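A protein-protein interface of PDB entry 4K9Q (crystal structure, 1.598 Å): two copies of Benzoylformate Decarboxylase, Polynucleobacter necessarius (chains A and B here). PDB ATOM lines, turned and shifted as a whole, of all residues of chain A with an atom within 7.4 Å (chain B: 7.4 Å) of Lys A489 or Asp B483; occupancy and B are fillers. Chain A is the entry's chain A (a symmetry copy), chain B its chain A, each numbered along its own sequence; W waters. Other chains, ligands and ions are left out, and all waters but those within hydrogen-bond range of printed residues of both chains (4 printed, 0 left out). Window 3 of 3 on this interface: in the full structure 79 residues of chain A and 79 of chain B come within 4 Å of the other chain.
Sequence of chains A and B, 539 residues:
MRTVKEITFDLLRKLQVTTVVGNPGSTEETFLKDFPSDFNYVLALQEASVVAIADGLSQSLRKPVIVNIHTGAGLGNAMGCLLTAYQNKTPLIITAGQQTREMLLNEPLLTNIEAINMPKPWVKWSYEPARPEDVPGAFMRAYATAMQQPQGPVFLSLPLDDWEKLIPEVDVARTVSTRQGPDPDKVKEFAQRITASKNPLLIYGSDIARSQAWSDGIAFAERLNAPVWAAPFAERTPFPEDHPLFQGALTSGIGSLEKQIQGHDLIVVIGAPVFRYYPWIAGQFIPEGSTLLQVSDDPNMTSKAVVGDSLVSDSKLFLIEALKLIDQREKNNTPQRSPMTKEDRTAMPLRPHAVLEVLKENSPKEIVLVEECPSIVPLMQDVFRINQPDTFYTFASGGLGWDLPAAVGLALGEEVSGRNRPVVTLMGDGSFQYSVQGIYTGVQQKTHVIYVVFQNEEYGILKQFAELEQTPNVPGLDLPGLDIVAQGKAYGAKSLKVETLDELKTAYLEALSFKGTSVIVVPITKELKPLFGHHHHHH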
ATOM      1  N   ILE A 439      -1.387  17.764 -15.086  1.00  0.00           N
ATOM      2  CA  ILE A 439      -0.497  18.686 -14.376  1.00  0.00           C
ATOM      3  C   ILE A 439       0.496  19.349 -15.332  1.00  0.00           C
ATOM      4  O   ILE A 439       0.786  20.547 -15.225  1.00  0.00           O
ATOM      5  CB  ILE A 439       0.277  17.961 -13.255  1.00  0.00           C
ATOM      6  CG1 ILE A 439      -0.704  17.398 -12.220  1.00  0.00           C
ATOM      7  CG2 ILE A 439       1.264  18.906 -12.581  1.00  0.00           C
ATOM      8  CD1 ILE A 439      -0.031  16.519 -11.176  1.00  0.00           C
ATOM      9  N   TYR A 440       1.006  18.568 -16.279  1.00  0.00           N
ATOM     10  CA  TYR A 440       1.971  19.067 -17.243  1.00  0.00           C
ATOM     11  C   TYR A 440       1.452  20.300 -17.973  1.00  0.00           C
ATOM     12  O   TYR A 440       2.177  21.270 -18.169  1.00  0.00           O
ATOM     13  CB  TYR A 440       2.318  17.975 -18.250  1.00  0.00           C
ATOM     14  CG  TYR A 440       3.402  18.370 -19.231  1.00  0.00           C
ATOM     15  CD1 TYR A 440       4.722  18.540 -18.808  1.00  0.00           C
ATOM     16  CD2 TYR A 440       3.112  18.569 -20.574  1.00  0.00           C
ATOM     17  CE1 TYR A 440       5.720  18.899 -19.705  1.00  0.00           C
ATOM     18  CE2 TYR A 440       4.100  18.922 -21.479  1.00  0.00           C
ATOM     19  CZ  TYR A 440       5.398  19.089 -21.040  1.00  0.00           C
ATOM     20  OH  TYR A 440       6.359  19.442 -21.966  1.00  0.00           O
ATOM     21  N   ASP A 483       3.843   7.947  -4.288  1.00  0.00           N
ATOM     22  CA  ASP A 483       4.563   9.156  -3.881  1.00  0.00           C
ATOM     23  C   ASP A 483       4.018  10.290  -4.727  1.00  0.00           C
ATOM     24  O   ASP A 483       4.455  10.525  -5.860  1.00  0.00           O
ATOM     25  CB  ASP A 483       6.074   9.013  -4.084  1.00  0.00           C
ATOM     26  CG  ASP A 483       6.863  10.220  -3.554  1.00  0.00           C
ATOM     27  OD1 ASP A 483       6.269  11.306  -3.374  1.00  0.00           O
ATOM     28  OD2 ASP A 483       8.084  10.087  -3.321  1.00  0.00           O
ATOM     29  N   ILE A 484       3.029  10.980  -4.179  1.00  0.00           N
ATOM     30  CA  ILE A 484       2.336  12.001  -4.937  1.00  0.00           C
ATOM     31  C   ILE A 484       3.180  13.267  -5.085  1.00  0.00           C
ATOM     32  O   ILE A 484       3.042  13.984  -6.068  1.00  0.00           O
ATOM     33  CB  ILE A 484       0.953  12.266  -4.320  1.00  0.00           C
ATOM     34  CG1 ILE A 484       0.151  10.952  -4.352  1.00  0.00           C
ATOM     35  CG2 ILE A 484       0.223  13.373  -5.072  1.00  0.00           C
ATOM     36  CD1 ILE A 484      -1.260  11.062  -3.813  1.00  0.00           C
ATOM     37  N   VAL A 485       4.075  13.527  -4.130  1.00  0.00           N
ATOM     38  CA  VAL A 485       5.026  14.628  -4.296  1.00  0.00           C
ATOM     39  C   VAL A 485       5.855  14.406  -5.556  1.00  0.00           C
ATOM     40  O   VAL A 485       6.027  15.319  -6.364  1.00  0.00           O
ATOM     41  CB  VAL A 485       5.942  14.772  -3.073  1.00  0.00           C
ATOM     42  CG1 VAL A 485       7.044  15.801  -3.333  1.00  0.00           C
ATOM     43  CG2 VAL A 485       5.108  15.138  -1.840  1.00  0.00           C
ATOM     44  N   ALA A 486       6.336  13.178  -5.739  1.00  0.00           N
ATOM     45  CA  ALA A 486       7.106  12.840  -6.938  1.00  0.00           C
ATOM     46  C   ALA A 486       6.293  13.002  -8.217  1.00  0.00           C
ATOM     47  O   ALA A 486       6.849  13.354  -9.256  1.00  0.00           O
ATOM     48  CB  ALA A 486       7.685  11.430  -6.830  1.00  0.00           C
ATOM     49  N   GLN A 487       4.980  12.758  -8.151  1.00  0.00           N
ATOM     50  CA  GLN A 487       4.109  12.969  -9.316  1.00  0.00           C
ATOM     51  C   GLN A 487       4.074  14.439  -9.736  1.00  0.00           C
ATOM     52  O   GLN A 487       4.153  14.751 -10.924  1.00  0.00           O
ATOM     53  CB  GLN A 487       2.686  12.444  -9.066  1.00  0.00           C
ATOM     54  CG  GLN A 487       2.626  10.940  -8.927  1.00  0.00           C
ATOM     55  CD  GLN A 487       1.227  10.400  -8.655  1.00  0.00           C
ATOM     56  OE1 GLN A 487       0.375  11.077  -8.074  1.00  0.00           O
ATOM     57  NE2 GLN A 487       0.996   9.162  -9.065  1.00  0.00           N
ATOM     58  N   GLY A 488       3.966  15.336  -8.761  1.00  0.00           N
ATOM     59  CA  GLY A 488       4.038  16.761  -9.034  1.00  0.00           C
ATOM     60  C   GLY A 488       5.375  17.147  -9.656  1.00  0.00           C
ATOM     61  O   GLY A 488       5.424  17.880 -10.644  1.00  0.00           O
ATOM     62  N   LYS A 489       6.463  16.649  -9.070  1.00  0.00           N
ATOM     63  CA  LYS A 489       7.812  16.917  -9.565  1.00  0.00           C
ATOM     64  C   LYS A 489       7.987  16.407 -10.996  1.00  0.00           C
ATOM     65  O   LYS A 489       8.627  17.054 -11.829  1.00  0.00           O
ATOM     66  CB  LYS A 489       8.845  16.272  -8.633  1.00  0.00           C
ATOM     67  CG  LYS A 489      10.293  16.482  -9.050  1.00  0.00           C
ATOM     68  CD  LYS A 489      11.246  15.789  -8.085  1.00  0.00           C
ATOM     69  CE  LYS A 489      12.697  15.954  -8.520  1.00  0.00           C
ATOM     70  NZ  LYS A 489      13.654  15.365  -7.531  1.00  0.00           N
ATOM     71  N   ALA A 490       7.397  15.254 -11.281  1.00  0.00           N
ATOM     72  CA  ALA A 490       7.512  14.631 -12.593  1.00  0.00           C
ATOM     73  C   ALA A 490       7.070  15.576 -13.714  1.00  0.00           C
ATOM     74  O   ALA A 490       7.635  15.565 -14.803  1.00  0.00           O
ATOM     75  CB  ALA A 490       6.686  13.347 -12.630  1.00  0.00           C
ATOM     76  N   TYR A 491       6.056  16.389 -13.439  1.00  0.00           N
ATOM     77  CA  TYR A 491       5.489  17.270 -14.459  1.00  0.00           C
ATOM     78  C   TYR A 491       5.878  18.729 -14.269  1.00  0.00           C
ATOM     79  O   TYR A 491       5.377  19.608 -14.974  1.00  0.00           O
ATOM     80  CB  TYR A 491       3.972  17.110 -14.517  1.00  0.00           C
ATOM     81  CG  TYR A 491       3.580  15.745 -15.004  1.00  0.00           C
ATOM     82  CD1 TYR A 491       3.905  15.340 -16.293  1.00  0.00           C
ATOM     83  CD2 TYR A 491       2.927  14.852 -14.175  1.00  0.00           C
ATOM     84  CE1 TYR A 491       3.576  14.090 -16.752  1.00  0.00           C
ATOM     85  CE2 TYR A 491       2.581  13.588 -14.631  1.00  0.00           C
ATOM     86  CZ  TYR A 491       2.914  13.219 -15.919  1.00  0.00           C
ATOM     87  OH  TYR A 491       2.580  11.968 -16.382  1.00  0.00           O
ATOM     88  N   GLY A 492       6.760  18.971 -13.305  1.00  0.00           N
ATOM     89  CA  GLY A 492       7.349  20.292 -13.106  1.00  0.00           C
ATOM     90  C   GLY A 492       6.611  21.228 -12.158  1.00  0.00           C
ATOM     91  O   GLY A 492       6.939  22.417 -12.075  1.00  0.00           O
ATOM     92  N   ALA A 493       5.624  20.708 -11.433  1.00  0.00           N
ATOM     93  CA  ALA A 493       4.886  21.530 -10.476  1.00  0.00           C
ATOM     94  C   ALA A 493       5.663  21.727  -9.177  1.00  0.00           C
ATOM     95  O   ALA A 493       6.489  20.889  -8.805  1.00  0.00           O
ATOM     96  CB  ALA A 493       3.518  20.910 -10.176  1.00  0.00           C
ATOM     97  N   LYS A 494       5.411  22.846  -8.499  1.00  0.00           N
ATOM     98  CA  LYS A 494       5.841  23.002  -7.114  1.00  0.00           C
ATOM     99  C   LYS A 494       5.107  21.911  -6.355  1.00  0.00           C
ATOM    100  O   LYS A 494       3.891  21.768  -6.495  1.00  0.00           O
ATOM    101  CB  LYS A 494       5.450  24.377  -6.573  1.00  0.00           C
ATOM    102  CG  LYS A 494       6.215  25.522  -7.177  1.00  0.00           C
ATOM    103  CD  LYS A 494       7.704  25.389  -6.915  1.00  0.00           C
ATOM    104  CE  LYS A 494       8.448  26.643  -7.355  1.00  0.00           C
ATOM    105  NZ  LYS A 494       7.950  27.845  -6.618  1.00  0.00           N
ATOM    106  N   SER A 495       5.826  21.118  -5.576  1.00  0.00           N
ATOM    107  CA  SER A 495       5.240  19.930  -4.969  1.00  0.00           C
ATOM    108  C   SER A 495       5.850  19.643  -3.598  1.00  0.00           C
ATOM    109  O   SER A 495       7.075  19.616  -3.455  1.00  0.00           O
ATOM    110  CB  SER A 495       5.473  18.737  -5.901  1.00  0.00           C
ATOM    111  OG  SER A 495       4.748  17.594  -5.498  1.00  0.00           O
ATOM    112  N   LEU A 496       5.010  19.413  -2.600  1.00  0.00           N
ATOM    113  CA  LEU A 496       5.512  19.040  -1.285  1.00  0.00           C
ATOM    114  C   LEU A 496       4.427  18.379  -0.462  1.00  0.00           C
ATOM    115  O   LEU A 496       3.232  18.502  -0.760  1.00  0.00           O
ATOM    116  CB  LEU A 496       6.059  20.255  -0.536  1.00  0.00           C
ATOM    117  CG  LEU A 496       5.017  21.120   0.169  1.00  0.00           C
ATOM    118  CD1 LEU A 496       5.677  22.019   1.223  1.00  0.00           C
ATOM    119  CD2 LEU A 496       4.276  21.931  -0.859  1.00  0.00           C
ATOM    120  N   VAL A 519       1.332  21.437  -6.102  1.00  0.00           N
ATOM    121  CA  VAL A 519       0.718  20.264  -5.493  1.00  0.00           C
ATOM    122  C   VAL A 519       1.070  20.225  -4.008  1.00  0.00           C
ATOM    123  O   VAL A 519       2.247  20.270  -3.632  1.00  0.00           O
ATOM    124  CB  VAL A 519       1.179  18.964  -6.186  1.00  0.00           C
ATOM    125  CG1 VAL A 519       0.606  17.734  -5.489  1.00  0.00           C
ATOM    126  CG2 VAL A 519       0.773  18.987  -7.648  1.00  0.00           C
ATOM    127  N   PHE B 432       5.485   7.039 -23.152  1.00  0.00           N
ATOM    128  CA  PHE B 432       5.508   6.676 -21.729  1.00  0.00           C
ATOM    129  C   PHE B 432       4.387   7.350 -20.933  1.00  0.00           C
ATOM    130  O   PHE B 432       3.865   6.774 -19.979  1.00  0.00           O
ATOM    131  CB  PHE B 432       6.870   7.078 -21.151  1.00  0.00           C
ATOM    132  CG  PHE B 432       7.220   6.428 -19.832  1.00  0.00           C
ATOM    133  CD1 PHE B 432       7.637   5.103 -19.780  1.00  0.00           C
ATOM    134  CD2 PHE B 432       7.205   7.168 -18.660  1.00  0.00           C
ATOM    135  CE1 PHE B 432       7.997   4.523 -18.568  1.00  0.00           C
ATOM    136  CE2 PHE B 432       7.572   6.595 -17.448  1.00  0.00           C
ATOM    137  CZ  PHE B 432       7.961   5.275 -17.408  1.00  0.00           C
ATOM    138  N   GLN B 433       4.012   8.568 -21.331  1.00  0.00           N
ATOM    139  CA  GLN B 433       3.032   9.359 -20.576  1.00  0.00           C
ATOM    140  C   GLN B 433       1.590   8.874 -20.657  1.00  0.00           C
ATOM    141  O   GLN B 433       0.815   9.097 -19.732  1.00  0.00           O
ATOM    142  CB  GLN B 433       3.052  10.820 -21.041  1.00  0.00           C
ATOM    143  CG  GLN B 433       4.439  11.441 -21.105  1.00  0.00           C
ATOM    144  CD  GLN B 433       5.147  11.367 -19.773  1.00  0.00           C
ATOM    145  OE1 GLN B 433       4.554  11.660 -18.730  1.00  0.00           O
ATOM    146  NE2 GLN B 433       6.412  10.942 -19.791  1.00  0.00           N
ATOM    147  N   GLN B 455      14.797   9.233 -24.106  1.00  0.00           N
ATOM    148  CA  GLN B 455      14.358  10.606 -23.888  1.00  0.00           C
ATOM    149  C   GLN B 455      14.964  11.611 -24.874  1.00  0.00           C
ATOM    150  O   GLN B 455      16.082  12.080 -24.684  1.00  0.00           O
ATOM    151  CB  GLN B 455      14.606  11.036 -22.437  1.00  0.00           C
ATOM    152  CG  GLN B 455      14.054  12.416 -22.143  1.00  0.00           C
ATOM    153  CD  GLN B 455      14.193  12.810 -20.696  1.00  0.00           C
ATOM    154  OE1 GLN B 455      15.295  12.842 -20.146  1.00  0.00           O
ATOM    155  NE2 GLN B 455      13.077  13.135 -20.073  1.00  0.00           N
ATOM    156  N   PRO B 480       9.546  19.494 -23.332  1.00  0.00           N
ATOM    157  CA  PRO B 480      10.470  19.898 -22.271  1.00  0.00           C
ATOM    158  C   PRO B 480       9.889  19.681 -20.878  1.00  0.00           C
ATOM    159  O   PRO B 480       8.668  19.548 -20.699  1.00  0.00           O
ATOM    160  CB  PRO B 480      10.633  21.400 -22.522  1.00  0.00           C
ATOM    161  CG  PRO B 480       9.313  21.795 -23.098  1.00  0.00           C
ATOM    162  CD  PRO B 480       8.970  20.657 -24.023  1.00  0.00           C
ATOM    163  N   GLY B 481      10.772  19.644 -19.892  1.00  0.00           N
ATOM    164  CA  GLY B 481      10.347  19.646 -18.507  1.00  0.00           C
ATOM    165  C   GLY B 481       9.642  18.415 -17.966  1.00  0.00           C
ATOM    166  O   GLY B 481       8.826  18.541 -17.064  1.00  0.00           O
ATOM    167  N   LEU B 482       9.932  17.231 -18.498  1.00  0.00           N
ATOM    168  CA  LEU B 482       9.430  16.001 -17.877  1.00  0.00           C
ATOM    169  C   LEU B 482      10.540  15.351 -17.077  1.00  0.00           C
ATOM    170  O   LEU B 482      11.648  15.161 -17.589  1.00  0.00           O
ATOM    171  CB  LEU B 482       8.930  15.005 -18.916  1.00  0.00           C
ATOM    172  CG  LEU B 482       7.734  15.444 -19.745  1.00  0.00           C
ATOM    173  CD1 LEU B 482       7.531  14.483 -20.902  1.00  0.00           C
ATOM    174  CD2 LEU B 482       6.496  15.531 -18.860  1.00  0.00           C
ATOM    175  N   ASP B 483      10.251  15.019 -15.820  1.00  0.00           N
ATOM    176  CA  ASP B 483      11.218  14.291 -14.995  1.00  0.00           C
ATOM    177  C   ASP B 483      10.723  12.860 -14.909  1.00  0.00           C
ATOM    178  O   ASP B 483       9.884  12.511 -14.068  1.00  0.00           O
ATOM    179  CB  ASP B 483      11.344  14.900 -13.595  1.00  0.00           C
ATOM    180  CG  ASP B 483      12.438  14.229 -12.751  1.00  0.00           C
ATOM    181  OD1 ASP B 483      12.842  13.089 -13.069  1.00  0.00           O
ATOM    182  OD2 ASP B 483      12.893  14.839 -11.759  1.00  0.00           O
ATOM    183  N   ILE B 484      11.225  12.032 -15.811  1.00  0.00           N
ATOM    184  CA  ILE B 484      10.735  10.674 -15.918  1.00  0.00           C
ATOM    185  C   ILE B 484      11.249   9.795 -14.778  1.00  0.00           C
ATOM    186  O   ILE B 484      10.579   8.847 -14.385  1.00  0.00           O
ATOM    187  CB  ILE B 484      11.056  10.107 -17.310  1.00  0.00           C
ATOM    188  CG1 ILE B 484      10.372  10.997 -18.364  1.00  0.00           C
ATOM    189  CG2 ILE B 484      10.592   8.659 -17.431  1.00  0.00           C
ATOM    190  CD1 ILE B 484      10.561  10.539 -19.795  1.00  0.00           C
ATOM    191  N   VAL B 485      12.418  10.122 -14.225  1.00  0.00           N
ATOM    192  CA  VAL B 485      12.883   9.425 -13.025  1.00  0.00           C
ATOM    193  C   VAL B 485      11.863   9.592 -11.905  1.00  0.00           C
ATOM    194  O   VAL B 485      11.495   8.624 -11.240  1.00  0.00           O
ATOM    195  CB  VAL B 485      14.259   9.933 -12.574  1.00  0.00           C
ATOM    196  CG1 VAL B 485      14.650   9.330 -11.223  1.00  0.00           C
ATOM    197  CG2 VAL B 485      15.305   9.628 -13.652  1.00  0.00           C
ATOM    198  N   ALA B 486      11.379  10.819 -11.724  1.00  0.00           N
ATOM    199  CA  ALA B 486      10.359  11.086 -10.708  1.00  0.00           C
ATOM    200  C   ALA B 486       9.065  10.324 -10.968  1.00  0.00           C
ATOM    201  O   ALA B 486       8.381   9.936 -10.022  1.00  0.00           O
ATOM    202  CB  ALA B 486      10.097  12.587 -10.584  1.00  0.00           C
ATOM    203  N   GLN B 487       8.725  10.097 -12.241  1.00  0.00           N
ATOM    204  CA  GLN B 487       7.537   9.300 -12.579  1.00  0.00           C
ATOM    205  C   GLN B 487       7.668   7.857 -12.090  1.00  0.00           C
ATOM    206  O   GLN B 487       6.722   7.298 -11.535  1.00  0.00           O
ATOM    207  CB  GLN B 487       7.239   9.334 -14.087  1.00  0.00           C
ATOM    208  CG  GLN B 487       6.820  10.703 -14.576  1.00  0.00           C
ATOM    209  CD  GLN B 487       6.541  10.765 -16.073  1.00  0.00           C
ATOM    210  OE1 GLN B 487       7.102  10.005 -16.866  1.00  0.00           O
ATOM    211  NE2 GLN B 487       5.678  11.691 -16.462  1.00  0.00           N
ATOM    212  N   GLY B 488       8.841   7.263 -12.287  1.00  0.00           N
ATOM    213  CA  GLY B 488       9.114   5.936 -11.763  1.00  0.00           C
ATOM    214  C   GLY B 488       9.006   5.901 -10.242  1.00  0.00           C
ATOM    215  O   GLY B 488       8.382   5.004  -9.674  1.00  0.00           O
ATOM    216  N   LYS B 489       9.620   6.883  -9.585  1.00  0.00           N
ATOM    217  CA  LYS B 489       9.589   6.991  -8.128  1.00  0.00           C
ATOM    218  C   LYS B 489       8.156   7.142  -7.615  1.00  0.00           C
ATOM    219  O   LYS B 489       7.784   6.572  -6.586  1.00  0.00           O
ATOM    220  CB  LYS B 489      10.451   8.175  -7.675  1.00  0.00           C
ATOM    221  CG  LYS B 489      10.494   8.390  -6.170  1.00  0.00           C
ATOM    222  CD  LYS B 489      11.349   9.598  -5.813  1.00  0.00           C
ATOM    223  CE  LYS B 489      11.361   9.849  -4.311  1.00  0.00           C
ATOM    224  NZ  LYS B 489      12.276  10.971  -3.931  1.00  0.00           N
ATOM    225  N   SER B 495      14.205   3.539 -10.195  1.00  0.00           N
ATOM    226  CA  SER B 495      14.196   4.557 -11.237  1.00  0.00           C
ATOM    227  C   SER B 495      15.481   5.384 -11.224  1.00  0.00           C
ATOM    228  O   SER B 495      15.893   5.877 -10.172  1.00  0.00           O
ATOM    229  CB  SER B 495      12.987   5.472 -11.018  1.00  0.00           C
ATOM    230  OG  SER B 495      12.776   6.349 -12.105  1.00  0.00           O
ATOM    231  N   LYS B 497      18.321   7.881 -14.043  1.00  0.00           N
ATOM    232  CA  LYS B 497      18.737   8.386 -15.339  1.00  0.00           C
ATOM    233  C   LYS B 497      20.212   8.065 -15.564  1.00  0.00           C
ATOM    234  O   LYS B 497      21.036   8.236 -14.656  1.00  0.00           O
ATOM    235  CB  LYS B 497      18.516   9.895 -15.379  1.00  0.00           C
ATOM    236  CG  LYS B 497      18.838  10.555 -16.709  1.00  0.00           C
ATOM    237  CD  LYS B 497      18.316  11.995 -16.705  1.00  0.00           C
ATOM    238  CE  LYS B 497      18.684  12.738 -17.968  1.00  0.00           C
ATOM    239  NZ  LYS B 497      18.331  14.185 -17.882  1.00  0.00           N
ATOM    240  N   VAL B 521      16.113   5.817 -17.554  1.00  0.00           N
ATOM    241  CA  VAL B 521      15.913   6.931 -18.475  1.00  0.00           C
ATOM    242  C   VAL B 521      17.228   7.227 -19.199  1.00  0.00           C
ATOM    243  O   VAL B 521      18.266   7.438 -18.562  1.00  0.00           O
ATOM    244  CB  VAL B 521      15.391   8.186 -17.721  1.00  0.00           C
ATOM    245  CG1 VAL B 521      15.137   9.337 -18.695  1.00  0.00           C
ATOM    246  CG2 VAL B 521      14.127   7.842 -16.916  1.00  0.00           C
HETATM  247  O   HOH W   1       9.991  18.341 -14.482  1.00  0.00           O
HETATM  248  O   HOH W   2       9.409  12.403  -3.072  1.00  0.00           O
HETATM  249  O   HOH W   3      14.252  13.287 -10.048  1.00  0.00           O
HETATM  250  O   HOH W   4       7.062  20.736 -16.930  1.00  0.00           O
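Hydrophobic or aromatic side chains of chain B that line the printed part of chain A: Pro B480, Leu B482 and Ala B486.
Among the printed residues, 13 pairs touch across the chains.
Among the printed residues, no Asp or Glu carboxylate lies within 4 Å of a Lys or Arg side-chain nitrogen of the other chain.
No residue of chain B comes within 4 Å of Gly A488.
Lys A489 touches one residue of chain B.
Of the printed residues of chain B, Ala A490 touches Gly B481, Leu B482, Asp B483, Ala B486 and Gln B487.
Gly A492 touches none of the printed residues of chain B.
Of the printed residues of chain A, Gln B433 touches Tyr A491 (3.1 Å).
Printed residues of chain A within 4 Å of Gly B481: Ala A490 (3.9 Å).
Asp B483 touches two residues of chain A.
Val B521 touches none of the printed residues of chain A.
The nearest residue of chain B that does not touch Lys A489 is Ala B486 (4.2 Å).
The nearest printed residue of chain A that does not touch Gln B433 is Ala A490 (6.3 Å).
The backbone NH of Asp B483 lies within hydrogen-bond range of the backbone carbonyl oxygen of Ala A490 (2.9 Å).
The backbone carbonyl oxygen (O) of Pro B480 is in hydrogen-bond range of the side-chain hydroxyl (OH) of Tyr A440, 2.6 Å away.
The side-chain amide nitrogen (NE2) of Gln B487 sits at hydrogen-bond distance from the side-chain hydroxyl (OH) of Tyr A491 (3.1 Å).
OH of Tyr A491 is in hydrogen-bond range of OE1 of Gln B433, at 3.1 Å.
Leu B482 touches Tyr A440 (CD2 to CD1, 3.5 Å).
CE of Lys B489 touches OD2 of Asp A483 (3.4 Å).
Ala B486 touches Ala A486 (CB to O, 3.6 Å).
CE of Lys A489 touches OD2 of Asp B483, 3.4 Å away.
Ala A490 touches Gly B481 (O to O, 3.9 Å).
Ala A490 touches Leu B482 (O to CA, 3.6 Å).
Ala B486 touches Ala A490.
Ala A490 touches Gln B487.
Tyr A491 touches Leu B482 (CD1 to CD2, 3.7 Å).
Asp A483 touches Lys B489, and with the chains exchanged Lys A489 touches Asp B483.
Ala A486 touches its own counterpart, Ala B486.
Positions printed for both chains: 483, 484, 485, 486, 487, 488, 489 and 495.
The side-chain carboxylate of Asp A483 lies within hydrogen-bond range of the backbone NH of Val A485, at 3.2 Å.
OD1 of Asp A483 is in hydrogen-bond range of N of Ala A486, at 3.0 Å.
OE1 of Gln B433 sits at hydrogen-bond distance from NE2 of Gln B487.
OD1 of Asp B483 lies within hydrogen-bond range of N of Val B485.
N of Ala B486 lies within hydrogen-bond range of OD1 of Asp B483 (3.0 Å).
Water W3 bridges OD2 of Asp B483 (2.7 Å) and NZ of Lys A489 (3.3 Å).
Water W2 lies within hydrogen-bond range of OD2 of Asp A483 (2.7 Å) and NZ of Lys B489 (3.3 Å).
Water W4 lies within hydrogen-bond range of O of Tyr A491 and O of Gly B481.
Water W1 lies within hydrogen-bond range of the backbone carbonyl oxygen (O) of Gly B481, the backbone carbonyl oxygen (O) of Lys A489 and the backbone NH (N) of Gly A492.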
